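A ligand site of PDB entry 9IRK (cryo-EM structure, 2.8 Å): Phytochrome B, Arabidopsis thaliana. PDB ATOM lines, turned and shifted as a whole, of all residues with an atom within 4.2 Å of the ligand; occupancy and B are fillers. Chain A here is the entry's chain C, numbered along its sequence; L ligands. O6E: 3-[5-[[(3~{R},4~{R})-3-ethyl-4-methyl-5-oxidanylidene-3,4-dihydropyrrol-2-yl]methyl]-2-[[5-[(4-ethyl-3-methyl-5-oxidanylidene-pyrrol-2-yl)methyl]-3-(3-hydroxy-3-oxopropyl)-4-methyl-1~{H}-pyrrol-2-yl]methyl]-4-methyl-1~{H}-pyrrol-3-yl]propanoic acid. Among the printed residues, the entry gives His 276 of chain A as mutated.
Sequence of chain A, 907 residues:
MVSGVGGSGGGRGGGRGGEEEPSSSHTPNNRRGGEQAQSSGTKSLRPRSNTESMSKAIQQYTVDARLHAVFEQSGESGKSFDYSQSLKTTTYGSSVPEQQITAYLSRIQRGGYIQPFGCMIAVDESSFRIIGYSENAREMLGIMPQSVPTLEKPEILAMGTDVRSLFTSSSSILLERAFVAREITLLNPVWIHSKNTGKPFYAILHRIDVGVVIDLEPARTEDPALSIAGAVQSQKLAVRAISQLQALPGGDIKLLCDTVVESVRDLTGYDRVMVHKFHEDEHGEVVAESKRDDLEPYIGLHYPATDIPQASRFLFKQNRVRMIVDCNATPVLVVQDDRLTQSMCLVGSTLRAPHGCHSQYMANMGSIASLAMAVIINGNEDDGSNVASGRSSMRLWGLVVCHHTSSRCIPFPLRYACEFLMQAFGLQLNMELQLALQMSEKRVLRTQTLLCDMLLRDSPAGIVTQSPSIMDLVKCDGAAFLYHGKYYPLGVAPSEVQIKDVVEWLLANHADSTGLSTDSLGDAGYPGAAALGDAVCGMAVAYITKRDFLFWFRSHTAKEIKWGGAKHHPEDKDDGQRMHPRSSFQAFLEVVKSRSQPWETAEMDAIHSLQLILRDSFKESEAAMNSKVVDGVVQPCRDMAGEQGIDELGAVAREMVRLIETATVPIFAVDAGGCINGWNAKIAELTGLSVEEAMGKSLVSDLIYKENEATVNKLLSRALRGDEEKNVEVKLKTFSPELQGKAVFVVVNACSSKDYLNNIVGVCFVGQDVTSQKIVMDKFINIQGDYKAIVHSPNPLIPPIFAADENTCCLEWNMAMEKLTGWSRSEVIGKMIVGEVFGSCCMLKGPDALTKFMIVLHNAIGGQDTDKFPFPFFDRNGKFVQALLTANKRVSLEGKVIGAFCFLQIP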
ATOM      1  N   HIS A 276      27.941  12.267 -26.023  1.00  0.00           N
ATOM      2  CA  HIS A 276      27.614  13.679 -25.867  1.00  0.00           C
ATOM      3  C   HIS A 276      28.609  14.326 -24.912  1.00  0.00           C
ATOM      4  O   HIS A 276      28.818  13.826 -23.802  1.00  0.00           O
ATOM      5  CB  HIS A 276      26.198  13.839 -25.306  1.00  0.00           C
ATOM      6  CG  HIS A 276      25.112  13.495 -26.292  1.00  0.00           C
ATOM      7  ND1 HIS A 276      24.107  14.379 -26.609  1.00  0.00           N
ATOM      8  CD2 HIS A 276      24.900  12.391 -27.027  1.00  0.00           C
ATOM      9  CE1 HIS A 276      23.302  13.814 -27.489  1.00  0.00           C
ATOM     10  NE2 HIS A 276      23.764  12.608 -27.769  1.00  0.00           N
ATOM     11  N   LEU A 301      26.363  17.662 -34.207  1.00  0.00           N
ATOM     12  CA  LEU A 301      25.207  18.457 -33.820  1.00  0.00           C
ATOM     13  C   LEU A 301      25.499  19.214 -32.526  1.00  0.00           C
ATOM     14  O   LEU A 301      26.000  18.625 -31.562  1.00  0.00           O
ATOM     15  CB  LEU A 301      23.988  17.550 -33.644  1.00  0.00           C
ATOM     16  CG  LEU A 301      22.672  18.183 -33.176  1.00  0.00           C
ATOM     17  CD1 LEU A 301      22.046  18.979 -34.291  1.00  0.00           C
ATOM     18  CD2 LEU A 301      21.722  17.131 -32.677  1.00  0.00           C
ATOM     19  N   TYR A 303      23.448  21.687 -29.653  1.00  0.00           N
ATOM     20  CA  TYR A 303      22.112  22.027 -29.211  1.00  0.00           C
ATOM     21  C   TYR A 303      22.203  22.850 -27.938  1.00  0.00           C
ATOM     22  O   TYR A 303      23.221  22.803 -27.243  1.00  0.00           O
ATOM     23  CB  TYR A 303      21.247  20.782 -28.980  1.00  0.00           C
ATOM     24  CG  TYR A 303      21.807  19.762 -28.014  1.00  0.00           C
ATOM     25  CD1 TYR A 303      21.667  19.919 -26.651  1.00  0.00           C
ATOM     26  CD2 TYR A 303      22.452  18.622 -28.474  1.00  0.00           C
ATOM     27  CE1 TYR A 303      22.163  18.992 -25.774  1.00  0.00           C
ATOM     28  CE2 TYR A 303      22.953  17.685 -27.604  1.00  0.00           C
ATOM     29  CZ  TYR A 303      22.804  17.880 -26.252  1.00  0.00           C
ATOM     30  OH  TYR A 303      23.296  16.965 -25.367  1.00  0.00           O
ATOM     31  N   THR A 306      19.533  24.237 -22.533  1.00  0.00           N
ATOM     32  CA  THR A 306      18.255  24.084 -21.855  1.00  0.00           C
ATOM     33  C   THR A 306      17.520  22.818 -22.268  1.00  0.00           C
ATOM     34  O   THR A 306      16.432  22.559 -21.734  1.00  0.00           O
ATOM     35  CB  THR A 306      17.363  25.300 -22.134  1.00  0.00           C
ATOM     36  OG1 THR A 306      17.235  25.489 -23.553  1.00  0.00           O
ATOM     37  CG2 THR A 306      17.960  26.553 -21.514  1.00  0.00           C
ATOM     38  N   ASP A 307      18.079  22.019 -23.172  1.00  0.00           N
ATOM     39  CA  ASP A 307      17.441  20.768 -23.545  1.00  0.00           C
ATOM     40  C   ASP A 307      17.601  19.709 -22.453  1.00  0.00           C
ATOM     41  O   ASP A 307      16.836  18.745 -22.429  1.00  0.00           O
ATOM     42  CB  ASP A 307      18.012  20.251 -24.866  1.00  0.00           C
ATOM     43  CG  ASP A 307      17.615  21.112 -26.034  1.00  0.00           C
ATOM     44  OD1 ASP A 307      16.858  22.080 -25.831  1.00  0.00           O
ATOM     45  OD2 ASP A 307      18.045  20.818 -27.169  1.00  0.00           O
ATOM     46  N   ILE A 308      18.562  19.871 -21.566  1.00  0.00           N
ATOM     47  CA  ILE A 308      18.767  18.986 -20.426  1.00  0.00           C
ATOM     48  C   ILE A 308      18.737  19.827 -19.160  1.00  0.00           C
ATOM     49  O   ILE A 308      19.745  20.436 -18.785  1.00  0.00           O
ATOM     50  CB  ILE A 308      20.082  18.196 -20.542  1.00  0.00           C
ATOM     51  CG1 ILE A 308      20.196  17.529 -21.915  1.00  0.00           C
ATOM     52  CG2 ILE A 308      20.162  17.137 -19.472  1.00  0.00           C
ATOM     53  CD1 ILE A 308      21.543  16.920 -22.181  1.00  0.00           C
ATOM     54  N   PRO A 309      17.604  19.911 -18.470  1.00  0.00           N
ATOM     55  CA  PRO A 309      17.527  20.744 -17.275  1.00  0.00           C
ATOM     56  C   PRO A 309      18.611  20.414 -16.266  1.00  0.00           C
ATOM     57  O   PRO A 309      19.321  19.421 -16.391  1.00  0.00           O
ATOM     58  CB  PRO A 309      16.126  20.447 -16.727  1.00  0.00           C
ATOM     59  CG  PRO A 309      15.352  20.058 -17.902  1.00  0.00           C
ATOM     60  CD  PRO A 309      16.291  19.323 -18.805  1.00  0.00           C
ATOM     61  N   SER A 312      18.187  17.013 -14.127  1.00  0.00           N
ATOM     62  CA  SER A 312      18.669  15.799 -14.767  1.00  0.00           C
ATOM     63  C   SER A 312      20.177  15.649 -14.625  1.00  0.00           C
ATOM     64  O   SER A 312      20.680  14.550 -14.344  1.00  0.00           O
ATOM     65  CB  SER A 312      18.277  15.805 -16.246  1.00  0.00           C
ATOM     66  OG  SER A 312      16.876  15.871 -16.385  1.00  0.00           O
ATOM     67  N   PHE A 316      22.216  12.627 -12.704  1.00  0.00           N
ATOM     68  CA  PHE A 316      23.137  11.743 -13.403  1.00  0.00           C
ATOM     69  C   PHE A 316      24.424  11.520 -12.625  1.00  0.00           C
ATOM     70  O   PHE A 316      25.221  10.660 -13.012  1.00  0.00           O
ATOM     71  CB  PHE A 316      23.453  12.292 -14.785  1.00  0.00           C
ATOM     72  CG  PHE A 316      22.573  11.748 -15.869  1.00  0.00           C
ATOM     73  CD1 PHE A 316      22.683  10.436 -16.273  1.00  0.00           C
ATOM     74  CD2 PHE A 316      21.609  12.553 -16.464  1.00  0.00           C
ATOM     75  CE1 PHE A 316      21.873   9.930 -17.262  1.00  0.00           C
ATOM     76  CE2 PHE A 316      20.799  12.049 -17.443  1.00  0.00           C
ATOM     77  CZ  PHE A 316      20.931  10.737 -17.847  1.00  0.00           C
ATOM     78  N   ARG A 322      20.052   5.813 -16.605  1.00  0.00           N
ATOM     79  CA  ARG A 322      18.637   6.079 -16.828  1.00  0.00           C
ATOM     80  C   ARG A 322      18.180   5.191 -17.967  1.00  0.00           C
ATOM     81  O   ARG A 322      18.846   5.102 -18.996  1.00  0.00           O
ATOM     82  CB  ARG A 322      18.415   7.557 -17.164  1.00  0.00           C
ATOM     83  CG  ARG A 322      16.987   7.933 -17.551  1.00  0.00           C
ATOM     84  CD  ARG A 322      16.052   7.825 -16.371  1.00  0.00           C
ATOM     85  NE  ARG A 322      14.797   8.521 -16.623  1.00  0.00           N
ATOM     86  CZ  ARG A 322      13.637   8.212 -16.056  1.00  0.00           C
ATOM     87  NH1 ARG A 322      13.525   7.202 -15.210  1.00  0.00           N
ATOM     88  NH2 ARG A 322      12.558   8.924 -16.360  1.00  0.00           N
ATOM     89  N   ARG A 352      11.017   5.264 -12.384  1.00  0.00           N
ATOM     90  CA  ARG A 352      10.297   6.530 -12.497  1.00  0.00           C
ATOM     91  C   ARG A 352       9.942   6.817 -13.946  1.00  0.00           C
ATOM     92  O   ARG A 352      10.715   6.526 -14.858  1.00  0.00           O
ATOM     93  CB  ARG A 352      11.157   7.642 -11.907  1.00  0.00           C
ATOM     94  CG  ARG A 352      10.534   9.022 -11.955  1.00  0.00           C
ATOM     95  CD  ARG A 352      11.315   9.986 -11.089  1.00  0.00           C
ATOM     96  NE  ARG A 352      12.746   9.889 -11.324  1.00  0.00           N
ATOM     97  CZ  ARG A 352      13.377  10.441 -12.349  1.00  0.00           C
ATOM     98  NH1 ARG A 352      12.741  11.165 -13.247  1.00  0.00           N
ATOM     99  NH2 ARG A 352      14.694  10.260 -12.471  1.00  0.00           N
ATOM    100  N   HIS A 355       9.204  12.538 -18.299  1.00  0.00           N
ATOM    101  CA  HIS A 355       8.415  13.753 -18.348  1.00  0.00           C
ATOM    102  C   HIS A 355       7.667  13.867 -19.666  1.00  0.00           C
ATOM    103  O   HIS A 355       7.963  13.140 -20.626  1.00  0.00           O
ATOM    104  CB  HIS A 355       9.302  14.978 -18.149  1.00  0.00           C
ATOM    105  CG  HIS A 355       8.594  16.177 -17.613  1.00  0.00           C
ATOM    106  ND1 HIS A 355       8.711  17.429 -18.171  1.00  0.00           N
ATOM    107  CD2 HIS A 355       7.753  16.312 -16.558  1.00  0.00           C
ATOM    108  CE1 HIS A 355       7.969  18.282 -17.492  1.00  0.00           C
ATOM    109  NE2 HIS A 355       7.378  17.637 -16.504  1.00  0.00           N
ATOM    110  N   CYS A 357       7.680  16.623 -21.641  1.00  0.00           N
ATOM    111  CA  CYS A 357       8.574  17.267 -22.602  1.00  0.00           C
ATOM    112  C   CYS A 357       9.462  16.241 -23.295  1.00  0.00           C
ATOM    113  O   CYS A 357       9.511  16.168 -24.527  1.00  0.00           O
ATOM    114  CB  CYS A 357       9.417  18.322 -21.893  1.00  0.00           C
ATOM    115  SG  CYS A 357      10.149  19.616 -22.958  1.00  0.00           S
ATOM    116  N   HIS A 358      10.167  15.419 -22.503  1.00  0.00           N
ATOM    117  CA  HIS A 358      11.120  14.489 -23.096  1.00  0.00           C
ATOM    118  C   HIS A 358      10.414  13.332 -23.796  1.00  0.00           C
ATOM    119  O   HIS A 358      10.889  12.828 -24.811  1.00  0.00           O
ATOM    120  CB  HIS A 358      12.081  13.963 -22.026  1.00  0.00           C
ATOM    121  CG  HIS A 358      13.196  13.147 -22.584  1.00  0.00           C
ATOM    122  ND1 HIS A 358      13.943  13.533 -23.666  1.00  0.00           N
ATOM    123  CD2 HIS A 358      13.700  11.955 -22.184  1.00  0.00           C
ATOM    124  CE1 HIS A 358      14.849  12.612 -23.931  1.00  0.00           C
ATOM    125  NE2 HIS A 358      14.732  11.646 -23.044  1.00  0.00           N
ATOM    126  N   TYR A 361       9.487  14.706 -27.067  1.00  0.00           N
ATOM    127  CA  TYR A 361      10.696  14.838 -27.865  1.00  0.00           C
ATOM    128  C   TYR A 361      11.105  13.503 -28.475  1.00  0.00           C
ATOM    129  O   TYR A 361      11.430  13.420 -29.657  1.00  0.00           O
ATOM    130  CB  TYR A 361      11.822  15.399 -26.998  1.00  0.00           C
ATOM    131  CG  TYR A 361      13.002  15.925 -27.778  1.00  0.00           C
ATOM    132  CD1 TYR A 361      13.885  15.066 -28.401  1.00  0.00           C
ATOM    133  CD2 TYR A 361      13.248  17.288 -27.877  1.00  0.00           C
ATOM    134  CE1 TYR A 361      14.965  15.536 -29.115  1.00  0.00           C
ATOM    135  CE2 TYR A 361      14.324  17.769 -28.584  1.00  0.00           C
ATOM    136  CZ  TYR A 361      15.175  16.885 -29.201  1.00  0.00           C
ATOM    137  OH  TYR A 361      16.246  17.351 -29.915  1.00  0.00           O
ATOM    138  N   MET A 365      11.228  12.540 -32.439  1.00  0.00           N
ATOM    139  CA  MET A 365      12.495  12.123 -33.037  1.00  0.00           C
ATOM    140  C   MET A 365      12.393  10.722 -33.629  1.00  0.00           C
ATOM    141  O   MET A 365      13.131  10.385 -34.560  1.00  0.00           O
ATOM    142  CB  MET A 365      13.600  12.180 -31.996  1.00  0.00           C
ATOM    143  CG  MET A 365      14.883  11.488 -32.407  1.00  0.00           C
ATOM    144  SD  MET A 365      16.312  12.055 -31.485  1.00  0.00           S
ATOM    145  CE  MET A 365      15.637  12.162 -29.829  1.00  0.00           C
ATOM    146  N   SER A 370      15.272   4.105 -24.680  1.00  0.00           N
ATOM    147  CA  SER A 370      16.464   4.910 -24.426  1.00  0.00           C
ATOM    148  C   SER A 370      17.251   4.378 -23.234  1.00  0.00           C
ATOM    149  O   SER A 370      16.663   3.835 -22.294  1.00  0.00           O
ATOM    150  CB  SER A 370      16.081   6.367 -24.169  1.00  0.00           C
ATOM    151  OG  SER A 370      17.222   7.165 -23.893  1.00  0.00           O
ATOM    152  N   ALA A 372      20.767   5.899 -21.013  1.00  0.00           N
ATOM    153  CA  ALA A 372      21.757   6.944 -20.858  1.00  0.00           C
ATOM    154  C   ALA A 372      22.645   6.677 -19.641  1.00  0.00           C
ATOM    155  O   ALA A 372      22.149   6.320 -18.572  1.00  0.00           O
ATOM    156  CB  ALA A 372      21.094   8.313 -20.707  1.00  0.00           C
ATOM    157  N   HIS A 403      19.630   4.740 -28.531  1.00  0.00           N
ATOM    158  CA  HIS A 403      18.269   4.826 -29.046  1.00  0.00           C
ATOM    159  C   HIS A 403      17.927   3.584 -29.840  1.00  0.00           C
ATOM    160  O   HIS A 403      18.757   3.025 -30.576  1.00  0.00           O
ATOM    161  CB  HIS A 403      18.071   6.054 -29.957  1.00  0.00           C
ATOM    162  CG  HIS A 403      18.160   7.369 -29.239  1.00  0.00           C
ATOM    163  ND1 HIS A 403      17.409   7.656 -28.129  1.00  0.00           N
ATOM    164  CD2 HIS A 403      18.873   8.480 -29.510  1.00  0.00           C
ATOM    165  CE1 HIS A 403      17.674   8.879 -27.725  1.00  0.00           C
ATOM    166  NE2 HIS A 403      18.574   9.401 -28.550  1.00  0.00           N
HETATM  167  CAH O6E L   1      11.572  20.916 -21.454  1.00  0.00           C
HETATM  168  CAC O6E L   1      11.810  20.361 -22.937  1.00  0.00           C
HETATM  169  CBJ O6E L   1      13.271  20.613 -23.131  1.00  0.00           C
HETATM  170  CBD O6E L   1      13.514  20.629 -24.641  1.00  0.00           C
HETATM  171  CAT O6E L   1      14.114  21.900 -25.175  1.00  0.00           C
HETATM  172  CAX O6E L   1      14.278  19.357 -24.878  1.00  0.00           C
HETATM  173  OBQ O6E L   1      14.773  19.037 -25.932  1.00  0.00           O
HETATM  174  NBP O6E L   1      14.287  18.605 -23.736  1.00  0.00           N
HETATM  175  CBN O6E L   1      13.834  19.320 -22.620  1.00  0.00           C
HETATM  176  CAQ O6E L   1      13.757  18.838 -21.303  1.00  0.00           C
HETATM  177  CAY O6E L   1      14.240  17.604 -20.769  1.00  0.00           C
HETATM  178  NAN O6E L   1      15.301  16.890 -21.272  1.00  0.00           N
HETATM  179  CBE O6E L   1      13.846  16.917 -19.579  1.00  0.00           C
HETATM  180  CAU O6E L   1      12.724  17.330 -18.676  1.00  0.00           C
HETATM  181  CBK O6E L   1      14.656  15.821 -19.427  1.00  0.00           C
HETATM  182  CAD O6E L   1      14.570  14.783 -18.356  1.00  0.00           C
HETATM  183  CAI O6E L   1      13.621  13.667 -18.760  1.00  0.00           C
HETATM  184  CAM O6E L   1      13.636  12.481 -17.823  1.00  0.00           C
HETATM  185  OBG O6E L   1      12.951  12.537 -16.796  1.00  0.00           O
HETATM  186  OBA O6E L   1      14.328  11.510 -18.131  1.00  0.00           O
HETATM  187  CBO O6E L   1      15.561  15.807 -20.492  1.00  0.00           C
HETATM  188  CAO O6E L   1      16.543  14.890 -20.757  1.00  0.00           C
HETATM  189  CAV O6E L   1      17.252  14.779 -21.903  1.00  0.00           C
HETATM  190  NAE O6E L   1      16.956  15.457 -23.042  1.00  0.00           N
HETATM  191  CBB O6E L   1      18.421  13.952 -22.095  1.00  0.00           C
HETATM  192  CAA O6E L   1      19.107  13.133 -21.046  1.00  0.00           C
HETATM  193  CAF O6E L   1      18.887  11.633 -21.200  1.00  0.00           C
HETATM  194  CAL O6E L   1      17.630  11.098 -20.564  1.00  0.00           C
HETATM  195  OBF O6E L   1      17.282  11.522 -19.442  1.00  0.00           O
HETATM  196  OAZ O6E L   1      16.988  10.247 -21.189  1.00  0.00           O
HETATM  197  CBH O6E L   1      18.768  14.102 -23.391  1.00  0.00           C
HETATM  198  CAR O6E L   1      19.807  13.312 -24.133  1.00  0.00           C
HETATM  199  CBL O6E L   1      17.975  15.199 -23.905  1.00  0.00           C
HETATM  200  CAP O6E L   1      18.220  15.912 -25.022  1.00  0.00           C
HETATM  201  CAW O6E L   1      18.471  15.435 -26.246  1.00  0.00           C
HETATM  202  CBC O6E L   1      18.869  16.201 -27.363  1.00  0.00           C
HETATM  203  CAS O6E L   1      18.840  17.689 -27.511  1.00  0.00           C
HETATM  204  NAJ O6E L   1      18.388  14.136 -26.626  1.00  0.00           N
HETATM  205  CBM O6E L   1      19.052  13.972 -27.801  1.00  0.00           C
HETATM  206  OAK O6E L   1      19.358  12.908 -28.288  1.00  0.00           O
HETATM  207  CBI O6E L   1      19.317  15.291 -28.343  1.00  0.00           C
HETATM  208  CAB O6E L   1      19.878  15.545 -29.569  1.00  0.00           C
HETATM  209  CAG O6E L   1      20.092  14.650 -30.486  1.00  0.00           C
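The guanidinium group (NE) of Arg 322 is in salt-bridge range of an oxygen (OBA) of the ligand. The backbone carbonyl oxygen (O) of Asp 307 lies within hydrogen-bond range of a nitrogen (NAN) of the ligand, at 2.7 Å. NH1 of Arg 352 is in salt-bridge range of OBG of the ligand, 3.8 Å away. OAZ of the ligand sits at hydrogen-bond distance from NE2 of His 358. The side-chain sulfur (SG) of Cys 357 is bonded to a carbon (CAC) of the ligand, at 1.8 Å.
A ring nitrogen (ND1) of His 276 lies within hydrogen-bond range of the side-chain hydroxyl (OH) of Tyr 303. The backbone NH (N) of Ala 372 sits at hydrogen-bond distance from the backbone carbonyl oxygen (O) of Arg 322, at 2.9 Å. The backbone carbonyl oxygen of Arg 352 lies within hydrogen-bond range of the guanidinium group of Arg 322 (2.9 Å).
Residues that only touch the ligand: Tyr 361 (3.0 Å), Ser 312 (3.2 Å), Pro 309 (3.3 Å), His 403 (3.6 Å), Tyr 303 (3.7 Å), Leu 301 (3.7 Å), Ile 308 (3.8 Å) and Thr 306 (3.97 Å). Hydrophobic or aromatic side chains that line the ligand: Leu 301, Tyr 303, Ile 308, Pro 309, His 358 and Tyr 361. The nearest printed residue that does not touch the ligand is Ala 372 (4.02 Å).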
